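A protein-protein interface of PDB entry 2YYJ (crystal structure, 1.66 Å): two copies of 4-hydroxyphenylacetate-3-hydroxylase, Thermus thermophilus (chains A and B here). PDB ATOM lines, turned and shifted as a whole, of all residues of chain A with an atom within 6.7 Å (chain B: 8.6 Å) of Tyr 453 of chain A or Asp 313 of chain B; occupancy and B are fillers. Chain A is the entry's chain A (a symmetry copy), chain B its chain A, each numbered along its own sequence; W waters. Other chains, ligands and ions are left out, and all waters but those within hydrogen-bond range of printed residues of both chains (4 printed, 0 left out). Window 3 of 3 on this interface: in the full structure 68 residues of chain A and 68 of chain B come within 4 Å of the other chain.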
ATOM      1  N   MET A 448       1.543  19.486 -10.656  1.00  0.00           N
ATOM      2  CA  MET A 448       0.275  18.792 -10.458  1.00  0.00           C
ATOM      3  C   MET A 448      -0.370  19.373  -9.200  1.00  0.00           C
ATOM      4  O   MET A 448      -1.583  19.571  -9.148  1.00  0.00           O
ATOM      5  CB  MET A 448       0.483  17.285 -10.272  1.00  0.00           C
ATOM      6  CG  MET A 448       0.786  16.534 -11.557  1.00  0.00           C
ATOM      7  SD  MET A 448       0.991  14.768 -11.277  1.00  0.00           S
ATOM      8  CE  MET A 448      -0.684  14.282 -10.880  1.00  0.00           C
ATOM      9  N   TYR A 449       0.448  19.644  -8.186  1.00  0.00           N
ATOM     10  CA  TYR A 449      -0.070  20.206  -6.944  1.00  0.00           C
ATOM     11  C   TYR A 449      -0.515  21.650  -7.139  1.00  0.00           C
ATOM     12  O   TYR A 449      -1.542  22.068  -6.600  1.00  0.00           O
ATOM     13  CB  TYR A 449       0.977  20.095  -5.831  1.00  0.00           C
ATOM     14  CG  TYR A 449       0.888  18.782  -5.080  1.00  0.00           C
ATOM     15  CD1 TYR A 449       0.988  17.560  -5.748  1.00  0.00           C
ATOM     16  CD2 TYR A 449       0.661  18.762  -3.703  1.00  0.00           C
ATOM     17  CE1 TYR A 449       0.860  16.352  -5.064  1.00  0.00           C
ATOM     18  CE2 TYR A 449       0.529  17.559  -3.009  1.00  0.00           C
ATOM     19  CZ  TYR A 449       0.628  16.360  -3.692  1.00  0.00           C
ATOM     20  OH  TYR A 449       0.484  15.174  -3.000  1.00  0.00           O
ATOM     21  N   GLN A 450       0.251  22.416  -7.911  1.00  0.00           N
ATOM     22  CA  GLN A 450      -0.129  23.799  -8.180  1.00  0.00           C
ATOM     23  C   GLN A 450      -1.445  23.806  -8.962  1.00  0.00           C
ATOM     24  O   GLN A 450      -2.301  24.669  -8.749  1.00  0.00           O
ATOM     25  CB  GLN A 450       0.976  24.505  -8.966  1.00  0.00           C
ATOM     26  CG  GLN A 450       2.166  24.879  -8.099  1.00  0.00           C
ATOM     27  CD  GLN A 450       3.366  25.336  -8.905  1.00  0.00           C
ATOM     28  OE1 GLN A 450       3.231  25.775 -10.046  1.00  0.00           O
ATOM     29  NE2 GLN A 450       4.547  25.250  -8.306  1.00  0.00           N
ATOM     30  N   THR A 451      -1.606  22.834  -9.858  1.00  0.00           N
ATOM     31  CA  THR A 451      -2.823  22.713 -10.655  1.00  0.00           C
ATOM     32  C   THR A 451      -4.011  22.431  -9.740  1.00  0.00           C
ATOM     33  O   THR A 451      -5.065  23.055  -9.866  1.00  0.00           O
ATOM     34  CB  THR A 451      -2.708  21.568 -11.695  1.00  0.00           C
ATOM     35  OG1 THR A 451      -1.787  21.947 -12.727  1.00  0.00           O
ATOM     36  CG2 THR A 451      -4.067  21.265 -12.319  1.00  0.00           C
ATOM     37  N   LEU A 452      -3.836  21.489  -8.816  1.00  0.00           N
ATOM     38  CA  LEU A 452      -4.906  21.141  -7.884  1.00  0.00           C
ATOM     39  C   LEU A 452      -5.299  22.357  -7.045  1.00  0.00           C
ATOM     40  O   LEU A 452      -6.482  22.639  -6.852  1.00  0.00           O
ATOM     41  CB  LEU A 452      -4.461  19.989  -6.975  1.00  0.00           C
ATOM     42  CG  LEU A 452      -5.443  19.550  -5.883  1.00  0.00           C
ATOM     43  CD1 LEU A 452      -6.777  19.157  -6.510  1.00  0.00           C
ATOM     44  CD2 LEU A 452      -4.852  18.383  -5.096  1.00  0.00           C
ATOM     45  N   TYR A 453      -4.303  23.085  -6.551  1.00  0.00           N
ATOM     46  CA  TYR A 453      -4.574  24.271  -5.748  1.00  0.00           C
ATOM     47  C   TYR A 453      -5.462  25.265  -6.495  1.00  0.00           C
ATOM     48  O   TYR A 453      -6.451  25.764  -5.960  1.00  0.00           O
ATOM     49  CB  TYR A 453      -3.267  24.977  -5.376  1.00  0.00           C
ATOM     50  CG  TYR A 453      -3.499  26.340  -4.762  1.00  0.00           C
ATOM     51  CD1 TYR A 453      -3.864  26.469  -3.422  1.00  0.00           C
ATOM     52  CD2 TYR A 453      -3.416  27.498  -5.539  1.00  0.00           C
ATOM     53  CE1 TYR A 453      -4.144  27.720  -2.870  1.00  0.00           C
ATOM     54  CE2 TYR A 453      -3.701  28.753  -4.995  1.00  0.00           C
ATOM     55  CZ  TYR A 453      -4.063  28.852  -3.661  1.00  0.00           C
ATOM     56  OH  TYR A 453      -4.350  30.086  -3.115  1.00  0.00           O
ATOM     57  N   ASN A 454      -5.102  25.555  -7.738  1.00  0.00           N
ATOM     58  CA  ASN A 454      -5.846  26.524  -8.528  1.00  0.00           C
ATOM     59  C   ASN A 454      -7.245  26.114  -8.969  1.00  0.00           C
ATOM     60  O   ASN A 454      -8.140  26.953  -9.037  1.00  0.00           O
ATOM     61  CB  ASN A 454      -5.013  26.942  -9.744  1.00  0.00           C
ATOM     62  CG  ASN A 454      -3.816  27.798  -9.357  1.00  0.00           C
ATOM     63  OD1 ASN A 454      -2.663  27.387  -9.503  1.00  0.00           O
ATOM     64  ND2 ASN A 454      -4.089  28.994  -8.847  1.00  0.00           N
ATOM     65  N   VAL A 455      -7.451  24.833  -9.250  1.00  0.00           N
ATOM     66  CA  VAL A 455      -8.762  24.387  -9.711  1.00  0.00           C
ATOM     67  C   VAL A 455      -9.752  24.041  -8.598  1.00  0.00           C
ATOM     68  O   VAL A 455     -10.963  24.153  -8.783  1.00  0.00           O
ATOM     69  CB  VAL A 455      -8.634  23.164 -10.658  1.00  0.00           C
ATOM     70  CG1 VAL A 455      -8.224  21.927  -9.876  1.00  0.00           C
ATOM     71  CG2 VAL A 455      -9.945  22.930 -11.384  1.00  0.00           C
ATOM     72  N   TYR A 456      -9.237  23.643  -7.441  1.00  0.00           N
ATOM     73  CA  TYR A 456     -10.089  23.250  -6.319  1.00  0.00           C
ATOM     74  C   TYR A 456     -10.906  24.407  -5.755  1.00  0.00           C
ATOM     75  O   TYR A 456     -10.413  25.526  -5.643  1.00  0.00           O
ATOM     76  CB  TYR A 456      -9.229  22.655  -5.200  1.00  0.00           C
ATOM     77  CG  TYR A 456      -9.967  21.696  -4.291  1.00  0.00           C
ATOM     78  CD1 TYR A 456     -10.283  20.407  -4.719  1.00  0.00           C
ATOM     79  CD2 TYR A 456     -10.319  22.062  -2.994  1.00  0.00           C
ATOM     80  CE1 TYR A 456     -10.921  19.498  -3.876  1.00  0.00           C
ATOM     81  CE2 TYR A 456     -10.962  21.162  -2.137  1.00  0.00           C
ATOM     82  CZ  TYR A 456     -11.256  19.881  -2.587  1.00  0.00           C
ATOM     83  OH  TYR A 456     -11.857  18.981  -1.737  1.00  0.00           O
ATOM     84  N   ASN A 457     -12.160  24.133  -5.404  1.00  0.00           N
ATOM     85  CA  ASN A 457     -13.020  25.155  -4.820  1.00  0.00           C
ATOM     86  C   ASN A 457     -12.759  25.190  -3.315  1.00  0.00           C
ATOM     87  O   ASN A 457     -13.232  24.332  -2.571  1.00  0.00           O
ATOM     88  CB  ASN A 457     -14.494  24.837  -5.088  1.00  0.00           C
ATOM     89  CG  ASN A 457     -15.432  25.817  -4.408  1.00  0.00           C
ATOM     90  OD1 ASN A 457     -15.028  26.920  -4.030  1.00  0.00           O
ATOM     91  ND2 ASN A 457     -16.694  25.425  -4.262  1.00  0.00           N
ATOM     92  N   LYS A 458     -12.006  26.194  -2.878  1.00  0.00           N
ATOM     93  CA  LYS A 458     -11.643  26.341  -1.474  1.00  0.00           C
ATOM     94  C   LYS A 458     -12.595  27.246  -0.692  1.00  0.00           C
ATOM     95  O   LYS A 458     -12.490  27.359   0.528  1.00  0.00           O
ATOM     96  CB  LYS A 458     -10.216  26.894  -1.385  1.00  0.00           C
ATOM     97  CG  LYS A 458      -9.176  26.021  -2.085  1.00  0.00           C
ATOM     98  CD  LYS A 458      -7.840  26.741  -2.264  1.00  0.00           C
ATOM     99  CE  LYS A 458      -7.927  27.861  -3.296  1.00  0.00           C
ATOM    100  NZ  LYS A 458      -8.243  27.345  -4.657  1.00  0.00           N
ATOM    101  N   LEU B 300      -7.732  23.454   6.170  1.00  0.00           N
ATOM    102  CA  LEU B 300      -7.655  23.897   4.780  1.00  0.00           C
ATOM    103  C   LEU B 300      -8.126  25.345   4.680  1.00  0.00           C
ATOM    104  O   LEU B 300      -7.493  26.169   4.018  1.00  0.00           O
ATOM    105  CB  LEU B 300      -8.527  23.014   3.886  1.00  0.00           C
ATOM    106  CG  LEU B 300      -8.702  23.491   2.439  1.00  0.00           C
ATOM    107  CD1 LEU B 300      -7.347  23.712   1.784  1.00  0.00           C
ATOM    108  CD2 LEU B 300      -9.509  22.454   1.670  1.00  0.00           C
ATOM    109  N   ALA B 303      -5.500  27.675   6.308  1.00  0.00           N
ATOM    110  CA  ALA B 303      -4.294  27.748   5.488  1.00  0.00           C
ATOM    111  C   ALA B 303      -4.526  28.654   4.279  1.00  0.00           C
ATOM    112  O   ALA B 303      -3.698  29.511   3.958  1.00  0.00           O
ATOM    113  CB  ALA B 303      -3.887  26.351   5.023  1.00  0.00           C
ATOM    114  N   ALA B 304      -5.661  28.464   3.612  1.00  0.00           N
ATOM    115  CA  ALA B 304      -5.993  29.261   2.438  1.00  0.00           C
ATOM    116  C   ALA B 304      -6.131  30.737   2.801  1.00  0.00           C
ATOM    117  O   ALA B 304      -5.590  31.602   2.109  1.00  0.00           O
ATOM    118  CB  ALA B 304      -7.286  28.746   1.804  1.00  0.00           C
ATOM    119  N   LEU B 305      -6.845  31.025   3.886  1.00  0.00           N
ATOM    120  CA  LEU B 305      -7.033  32.410   4.321  1.00  0.00           C
ATOM    121  C   LEU B 305      -5.723  33.066   4.753  1.00  0.00           C
ATOM    122  O   LEU B 305      -5.502  34.250   4.490  1.00  0.00           O
ATOM    123  CB  LEU B 305      -8.053  32.486   5.459  1.00  0.00           C
ATOM    124  CG  LEU B 305      -9.518  32.241   5.076  1.00  0.00           C
ATOM    125  CD1 LEU B 305     -10.389  32.322   6.321  1.00  0.00           C
ATOM    126  CD2 LEU B 305      -9.970  33.276   4.050  1.00  0.00           C
ATOM    127  N   MET B 306      -4.852  32.316   5.422  1.00  0.00           N
ATOM    128  CA  MET B 306      -3.576  32.890   5.837  1.00  0.00           C
ATOM    129  C   MET B 306      -2.745  33.244   4.610  1.00  0.00           C
ATOM    130  O   MET B 306      -2.207  34.346   4.516  1.00  0.00           O
ATOM    131  CB  MET B 306      -2.777  31.916   6.704  1.00  0.00           C
ATOM    132  CG  MET B 306      -3.036  32.040   8.191  1.00  0.00           C
ATOM    133  SD  MET B 306      -1.793  31.109   9.105  1.00  0.00           S
ATOM    134  CE  MET B 306      -2.351  29.515   8.733  1.00  0.00           C
ATOM    135  N   ALA B 307      -2.642  32.304   3.673  1.00  0.00           N
ATOM    136  CA  ALA B 307      -1.851  32.525   2.465  1.00  0.00           C
ATOM    137  C   ALA B 307      -2.357  33.733   1.688  1.00  0.00           C
ATOM    138  O   ALA B 307      -1.574  34.583   1.267  1.00  0.00           O
ATOM    139  CB  ALA B 307      -1.876  31.284   1.582  1.00  0.00           C
ATOM    140  N   GLU B 308      -3.668  33.807   1.494  1.00  0.00           N
ATOM    141  CA  GLU B 308      -4.252  34.935   0.779  1.00  0.00           C
ATOM    142  C   GLU B 308      -4.059  36.219   1.581  1.00  0.00           C
ATOM    143  O   GLU B 308      -3.729  37.270   1.028  1.00  0.00           O
ATOM    144  CB  GLU B 308      -5.746  34.706   0.554  1.00  0.00           C
ATOM    145  CG  GLU B 308      -6.071  33.711  -0.540  1.00  0.00           C
ATOM    146  CD  GLU B 308      -7.560  33.441  -0.646  1.00  0.00           C
ATOM    147  OE1 GLU B 308      -8.356  34.369  -0.377  1.00  0.00           O
ATOM    148  OE2 GLU B 308      -7.931  32.306  -1.013  1.00  0.00           O
ATOM    149  N   GLY B 309      -4.258  36.114   2.891  1.00  0.00           N
ATOM    150  CA  GLY B 309      -4.139  37.265   3.770  1.00  0.00           C
ATOM    151  C   GLY B 309      -2.826  38.020   3.729  1.00  0.00           C
ATOM    152  O   GLY B 309      -2.819  39.250   3.822  1.00  0.00           O
ATOM    153  N   ILE B 310      -1.714  37.307   3.598  1.00  0.00           N
ATOM    154  CA  ILE B 310      -0.412  37.964   3.563  1.00  0.00           C
ATOM    155  C   ILE B 310       0.238  37.947   2.183  1.00  0.00           C
ATOM    156  O   ILE B 310       1.414  38.280   2.044  1.00  0.00           O
ATOM    157  CB  ILE B 310       0.565  37.331   4.586  1.00  0.00           C
ATOM    158  CG1 ILE B 310       0.765  35.845   4.278  1.00  0.00           C
ATOM    159  CG2 ILE B 310       0.022  37.520   5.997  1.00  0.00           C
ATOM    160  CD1 ILE B 310       1.841  35.189   5.124  1.00  0.00           C
ATOM    161  N   GLY B 311      -0.530  37.560   1.168  1.00  0.00           N
ATOM    162  CA  GLY B 311      -0.011  37.531  -0.190  1.00  0.00           C
ATOM    163  C   GLY B 311       0.985  36.424  -0.488  1.00  0.00           C
ATOM    164  O   GLY B 311       1.709  36.487  -1.484  1.00  0.00           O
ATOM    165  N   ALA B 312       1.021  35.402   0.359  1.00  0.00           N
ATOM    166  CA  ALA B 312       1.943  34.293   0.158  1.00  0.00           C
ATOM    167  C   ALA B 312       1.417  33.276  -0.848  1.00  0.00           C
ATOM    168  O   ALA B 312       2.166  32.416  -1.314  1.00  0.00           O
ATOM    169  CB  ALA B 312       2.230  33.608   1.490  1.00  0.00           C
ATOM    170  N   ASP B 313       0.136  33.392  -1.194  1.00  0.00           N
ATOM    171  CA  ASP B 313      -0.496  32.466  -2.128  1.00  0.00           C
ATOM    172  C   ASP B 313       0.051  32.541  -3.553  1.00  0.00           C
ATOM    173  O   ASP B 313      -0.211  31.657  -4.369  1.00  0.00           O
ATOM    174  CB  ASP B 313      -2.019  32.683  -2.129  1.00  0.00           C
ATOM    175  CG  ASP B 313      -2.418  34.082  -2.580  1.00  0.00           C
ATOM    176  OD1 ASP B 313      -1.807  35.066  -2.117  1.00  0.00           O
ATOM    177  OD2 ASP B 313      -3.362  34.204  -3.389  1.00  0.00           O
ATOM    178  N   VAL B 314       0.819  33.584  -3.857  1.00  0.00           N
ATOM    179  CA  VAL B 314       1.386  33.728  -5.195  1.00  0.00           C
ATOM    180  C   VAL B 314       2.597  32.822  -5.403  1.00  0.00           C
ATOM    181  O   VAL B 314       3.041  32.620  -6.532  1.00  0.00           O
ATOM    182  CB  VAL B 314       1.806  35.195  -5.487  1.00  0.00           C
ATOM    183  CG1 VAL B 314       0.607  36.113  -5.332  1.00  0.00           C
ATOM    184  CG2 VAL B 314       2.937  35.625  -4.555  1.00  0.00           C
ATOM    185  N   TYR B 315       3.125  32.271  -4.314  1.00  0.00           N
ATOM    186  CA  TYR B 315       4.290  31.398  -4.399  1.00  0.00           C
ATOM    187  C   TYR B 315       3.921  29.934  -4.598  1.00  0.00           C
ATOM    188  O   TYR B 315       3.083  29.384  -3.886  1.00  0.00           O
ATOM    189  CB  TYR B 315       5.153  31.579  -3.150  1.00  0.00           C
ATOM    190  CG  TYR B 315       5.674  32.992  -3.059  1.00  0.00           C
ATOM    191  CD1 TYR B 315       6.602  33.464  -3.983  1.00  0.00           C
ATOM    192  CD2 TYR B 315       5.164  33.884  -2.119  1.00  0.00           C
ATOM    193  CE1 TYR B 315       7.007  34.795  -3.983  1.00  0.00           C
ATOM    194  CE2 TYR B 315       5.561  35.223  -2.107  1.00  0.00           C
ATOM    195  CZ  TYR B 315       6.481  35.668  -3.046  1.00  0.00           C
ATOM    196  OH  TYR B 315       6.863  36.989  -3.071  1.00  0.00           O
ATOM    197  N   GLY B 316       4.567  29.314  -5.581  1.00  0.00           N
ATOM    198  CA  GLY B 316       4.298  27.924  -5.901  1.00  0.00           C
ATOM    199  C   GLY B 316       4.296  26.947  -4.743  1.00  0.00           C
ATOM    200  O   GLY B 316       3.348  26.173  -4.584  1.00  0.00           O
ATOM    201  N   HIS B 317       5.338  26.977  -3.921  1.00  0.00           N
ATOM    202  CA  HIS B 317       5.415  26.033  -2.814  1.00  0.00           C
ATOM    203  C   HIS B 317       4.302  26.213  -1.788  1.00  0.00           C
ATOM    204  O   HIS B 317       3.917  25.255  -1.123  1.00  0.00           O
ATOM    205  CB  HIS B 317       6.800  26.093  -2.149  1.00  0.00           C
ATOM    206  CG  HIS B 317       6.994  27.264  -1.239  1.00  0.00           C
ATOM    207  ND1 HIS B 317       6.614  27.246   0.086  1.00  0.00           N
ATOM    208  CD2 HIS B 317       7.524  28.490  -1.463  1.00  0.00           C
ATOM    209  CE1 HIS B 317       6.899  28.412   0.638  1.00  0.00           C
ATOM    210  NE2 HIS B 317       7.451  29.185  -0.280  1.00  0.00           N
ATOM    211  N   VAL B 318       3.776  27.430  -1.663  1.00  0.00           N
ATOM    212  CA  VAL B 318       2.683  27.679  -0.727  1.00  0.00           C
ATOM    213  C   VAL B 318       1.424  27.040  -1.313  1.00  0.00           C
ATOM    214  O   VAL B 318       0.638  26.415  -0.599  1.00  0.00           O
ATOM    215  CB  VAL B 318       2.455  29.195  -0.512  1.00  0.00           C
ATOM    216  CG1 VAL B 318       1.208  29.427   0.329  1.00  0.00           C
ATOM    217  CG2 VAL B 318       3.672  29.800   0.182  1.00  0.00           C
ATOM    218  N   GLN B 319       1.243  27.191  -2.622  1.00  0.00           N
ATOM    219  CA  GLN B 319       0.098  26.594  -3.299  1.00  0.00           C
ATOM    220  C   GLN B 319       0.182  25.077  -3.152  1.00  0.00           C
ATOM    221  O   GLN B 319      -0.825  24.407  -2.913  1.00  0.00           O
ATOM    222  CB  GLN B 319       0.103  26.976  -4.781  1.00  0.00           C
ATOM    223  CG  GLN B 319      -0.005  28.474  -5.025  1.00  0.00           C
ATOM    224  CD  GLN B 319       0.038  28.831  -6.496  1.00  0.00           C
ATOM    225  OE1 GLN B 319       0.111  27.956  -7.358  1.00  0.00           O
ATOM    226  NE2 GLN B 319      -0.011  30.126  -6.789  1.00  0.00           N
ATOM    227  N   GLU B 320       1.392  24.537  -3.283  1.00  0.00           N
ATOM    228  CA  GLU B 320       1.599  23.097  -3.158  1.00  0.00           C
ATOM    229  C   GLU B 320       1.263  22.596  -1.756  1.00  0.00           C
ATOM    230  O   GLU B 320       0.677  21.523  -1.600  1.00  0.00           O
ATOM    231  CB  GLU B 320       3.045  22.742  -3.502  1.00  0.00           C
ATOM    232  CG  GLU B 320       3.397  23.001  -4.960  1.00  0.00           C
ATOM    233  CD  GLU B 320       4.890  23.050  -5.196  1.00  0.00           C
ATOM    234  OE1 GLU B 320       5.590  22.094  -4.798  1.00  0.00           O
ATOM    235  OE2 GLU B 320       5.363  24.049  -5.781  1.00  0.00           O
ATOM    236  N   LYS B 321       1.631  23.367  -0.735  1.00  0.00           N
ATOM    237  CA  LYS B 321       1.335  22.960   0.637  1.00  0.00           C
ATOM    238  C   LYS B 321      -0.171  22.921   0.876  1.00  0.00           C
ATOM    239  O   LYS B 321      -0.678  22.023   1.552  1.00  0.00           O
ATOM    240  CB  LYS B 321       2.001  23.910   1.639  1.00  0.00           C
ATOM    241  CG  LYS B 321       3.514  23.762   1.719  1.00  0.00           C
ATOM    242  CD  LYS B 321       4.129  24.856   2.584  1.00  0.00           C
ATOM    243  CE  LYS B 321       5.641  24.694   2.689  1.00  0.00           C
ATOM    244  NZ  LYS B 321       6.319  24.711   1.364  1.00  0.00           N
ATOM    245  N   ILE B 322      -0.893  23.887   0.318  1.00  0.00           N
ATOM    246  CA  ILE B 322      -2.339  23.911   0.491  1.00  0.00           C
ATOM    247  C   ILE B 322      -2.948  22.735  -0.273  1.00  0.00           C
ATOM    248  O   ILE B 322      -3.875  22.083   0.211  1.00  0.00           O
ATOM    249  CB  ILE B 322      -2.925  25.264   0.019  1.00  0.00           C
ATOM    250  CG1 ILE B 322      -2.445  26.369   0.971  1.00  0.00           C
ATOM    251  CG2 ILE B 322      -4.452  25.201  -0.023  1.00  0.00           C
ATOM    252  CD1 ILE B 322      -2.773  27.783   0.528  1.00  0.00           C
ATOM    253  N   ALA B 323      -2.406  22.442  -1.453  1.00  0.00           N
ATOM    254  CA  ALA B 323      -2.898  21.319  -2.248  1.00  0.00           C
ATOM    255  C   ALA B 323      -2.662  20.004  -1.500  1.00  0.00           C
ATOM    256  O   ALA B 323      -3.436  19.055  -1.630  1.00  0.00           O
ATOM    257  CB  ALA B 323      -2.197  21.289  -3.606  1.00  0.00           C
ATOM    258  N   GLU B 324      -1.590  19.950  -0.715  1.00  0.00           N
ATOM    259  CA  GLU B 324      -1.284  18.751   0.053  1.00  0.00           C
ATOM    260  C   GLU B 324      -2.412  18.512   1.064  1.00  0.00           C
ATOM    261  O   GLU B 324      -2.851  17.378   1.266  1.00  0.00           O
ATOM    262  CB  GLU B 324       0.058  18.917   0.774  1.00  0.00           C
ATOM    263  CG  GLU B 324       0.711  17.610   1.161  1.00  0.00           C
ATOM    264  CD  GLU B 324       2.077  17.806   1.794  1.00  0.00           C
ATOM    265  OE1 GLU B 324       2.846  18.663   1.307  1.00  0.00           O
ATOM    266  OE2 GLU B 324       2.382  17.090   2.768  1.00  0.00           O
ATOM    267  N   ILE B 326      -5.421  19.451   0.687  1.00  0.00           N
ATOM    268  CA  ILE B 326      -6.568  19.040  -0.117  1.00  0.00           C
ATOM    269  C   ILE B 326      -6.491  17.542  -0.411  1.00  0.00           C
ATOM    270  O   ILE B 326      -7.501  16.840  -0.361  1.00  0.00           O
ATOM    271  CB  ILE B 326      -6.627  19.829  -1.449  1.00  0.00           C
ATOM    272  CG1 ILE B 326      -6.944  21.299  -1.157  1.00  0.00           C
ATOM    273  CG2 ILE B 326      -7.693  19.238  -2.369  1.00  0.00           C
ATOM    274  CD1 ILE B 326      -6.769  22.220  -2.356  1.00  0.00           C
ATOM    275  N   VAL B 327      -5.291  17.054  -0.715  1.00  0.00           N
ATOM    276  CA  VAL B 327      -5.111  15.634  -0.994  1.00  0.00           C
ATOM    277  C   VAL B 327      -5.500  14.822   0.242  1.00  0.00           C
ATOM    278  O   VAL B 327      -6.208  13.817   0.139  1.00  0.00           O
ATOM    279  CB  VAL B 327      -3.642  15.316  -1.378  1.00  0.00           C
ATOM    280  CG1 VAL B 327      -3.425  13.804  -1.447  1.00  0.00           C
ATOM    281  CG2 VAL B 327      -3.313  15.952  -2.725  1.00  0.00           C
ATOM    282  N   ILE B 379       3.452  28.198   6.433  1.00  0.00           N
ATOM    283  CA  ILE B 379       2.773  29.267   5.701  1.00  0.00           C
ATOM    284  C   ILE B 379       2.737  30.557   6.519  1.00  0.00           C
ATOM    285  O   ILE B 379       3.054  31.632   6.011  1.00  0.00           O
ATOM    286  CB  ILE B 379       1.317  28.876   5.354  1.00  0.00           C
ATOM    287  CG1 ILE B 379       1.310  27.726   4.349  1.00  0.00           C
ATOM    288  CG2 ILE B 379       0.566  30.086   4.790  1.00  0.00           C
ATOM    289  CD1 ILE B 379      -0.082  27.158   4.109  1.00  0.00           C
ATOM    290  N   ALA B 408      -2.596  41.903   2.714  1.00  0.00           N
ATOM    291  CA  ALA B 408      -2.585  42.372   1.331  1.00  0.00           C
ATOM    292  C   ALA B 408      -3.862  43.154   1.016  1.00  0.00           C
ATOM    293  O   ALA B 408      -3.812  44.273   0.506  1.00  0.00           O
ATOM    294  CB  ALA B 408      -2.443  41.186   0.382  1.00  0.00           C
HETATM  295  O   HOH W   1      -6.620  29.992  -1.341  1.00  0.00           O
HETATM  296  O   HOH W   2      -2.203  30.864  -9.256  1.00  0.00           O
HETATM  297  O   HOH W   3      -4.688  32.282  -4.604  1.00  0.00           O
HETATM  298  O   HOH W   4       1.422  28.368  -9.693  1.00  0.00           O
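Glu 320 of chain B touches Tyr 449 of chain A. CB of Ala 323 of chain B touches O of Tyr 449 of chain A (3.2 Å). CA of Glu 324 of chain B touches CE2 of Tyr 449 of chain A, at 3.8 Å. Val 327 of chain B touches Tyr 449 of chain A. CG of Gln 450 of chain A touches OE1 of Gln 319 of chain B (3.8 Å). Leu 452 of chain A touches Ala 323 of chain B. CD2 of Leu 452 of chain A touches CG2 of Val 327 of chain B, at 3.7 Å. Tyr 453 of chain A touches Asp 313 of chain B (OH to CB, 3.6 Å). OD1 of Asn 454 of chain A touches OE1 of Gln 319 of chain B (3.6 Å). Tyr 456 of chain A touches Ile 326 of chain B.
No position is printed for both chains. Of the 14 pairs that touch across the chains among the printed residues, none has its exchanged pair printed and touching as well.
Along chain B the printed residues that touch a printed residue of chain A span positions 313 to 327. Printed residues of chain A that touch a printed residue of chain B: Tyr 449, Gln 450, Leu 452, Tyr 453, Asn 454 and Tyr 456. Hydrophobic or aromatic side chains of chain A within 4 Å of the printed part of chain B: Tyr 449, Leu 452, Tyr 453 and Tyr 456.
Water W3 bridges OD2 of Asp 313 of chain B and OH of Tyr 453 of chain A. Water W1 bridges OE2 of Glu 308 of chain B and OH of Tyr 453 of chain A. Water W2 bridges the side-chain amide nitrogen of Asn 454 of chain A and the side-chain amide nitrogen of Gln 319 of chain B. Water W4 lies within hydrogen-bond range of the side-chain amide oxygen of Gln 319 of chain B (2.7 Å) and the side-chain amide oxygen of Gln 450 of chain A (3.2 Å).
The side-chain amide nitrogen (NE2) of Gln 450 of chain A is in hydrogen-bond range of the side-chain carboxylate (OE2) of Glu 320 of chain B (2.9 Å).
Of chain B, only Asp 313, Gln 319 and Ile 322 come within 4 Å of Tyr 453 of chain A. Of chain A, only Tyr 453 comes within 4 Å of Asp 313 of chain B. Of the printed residues of chain B, Leu 452 of chain A touches Ala 323 and Val 327. Printed residues of chain A within 4 Å of Gly 316 of chain B: Gln 450. Of the printed residues of chain A, Ala 323 of chain B touches Tyr 449 (3.2 Å) and Leu 452 (3.8 Å). Printed residues of chain B within 4 Å of Tyr 456 of chain A: Ile 326 (3.6 Å). Printed residues of chain A within 4 Å of Ile 322 of chain B: Tyr 453 (3.7 Å). Val 455 of chain A touches none of the printed residues of chain B. Gly 309 of chain B touches none of the printed residues of chain A. The nearest printed residue of chain B that does not touch Tyr 456 of chain A is Leu 300 of chain B (4.3 Å).
NZ of Lys 458 of chain A sits at hydrogen-bond distance from O of Tyr 456 of chain A, at 3.0 Å. The backbone carbonyl oxygen (O) of Tyr 453 of chain A sits at hydrogen-bond distance from the side-chain amino group (NZ) of Lys 458 of chain A, 2.7 Å away. The backbone NH (N) of His 317 of chain B sits at hydrogen-bond distance from the side-chain carboxylate (OE2) of Glu 320 of chain B (3.5 Å). The backbone NH (N) of Asp 313 of chain B is in hydrogen-bond range of the backbone carbonyl oxygen (O) of Ala 307 of chain B, at 3.2 Å. The backbone carbonyl oxygen of Asp 313 of chain B lies within hydrogen-bond range of the side-chain amide nitrogen of Gln 319 of chain B (2.9 Å). O of Gln 450 of chain A sits close to OD1 of Asn 454 of chain A (2.8 Å).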
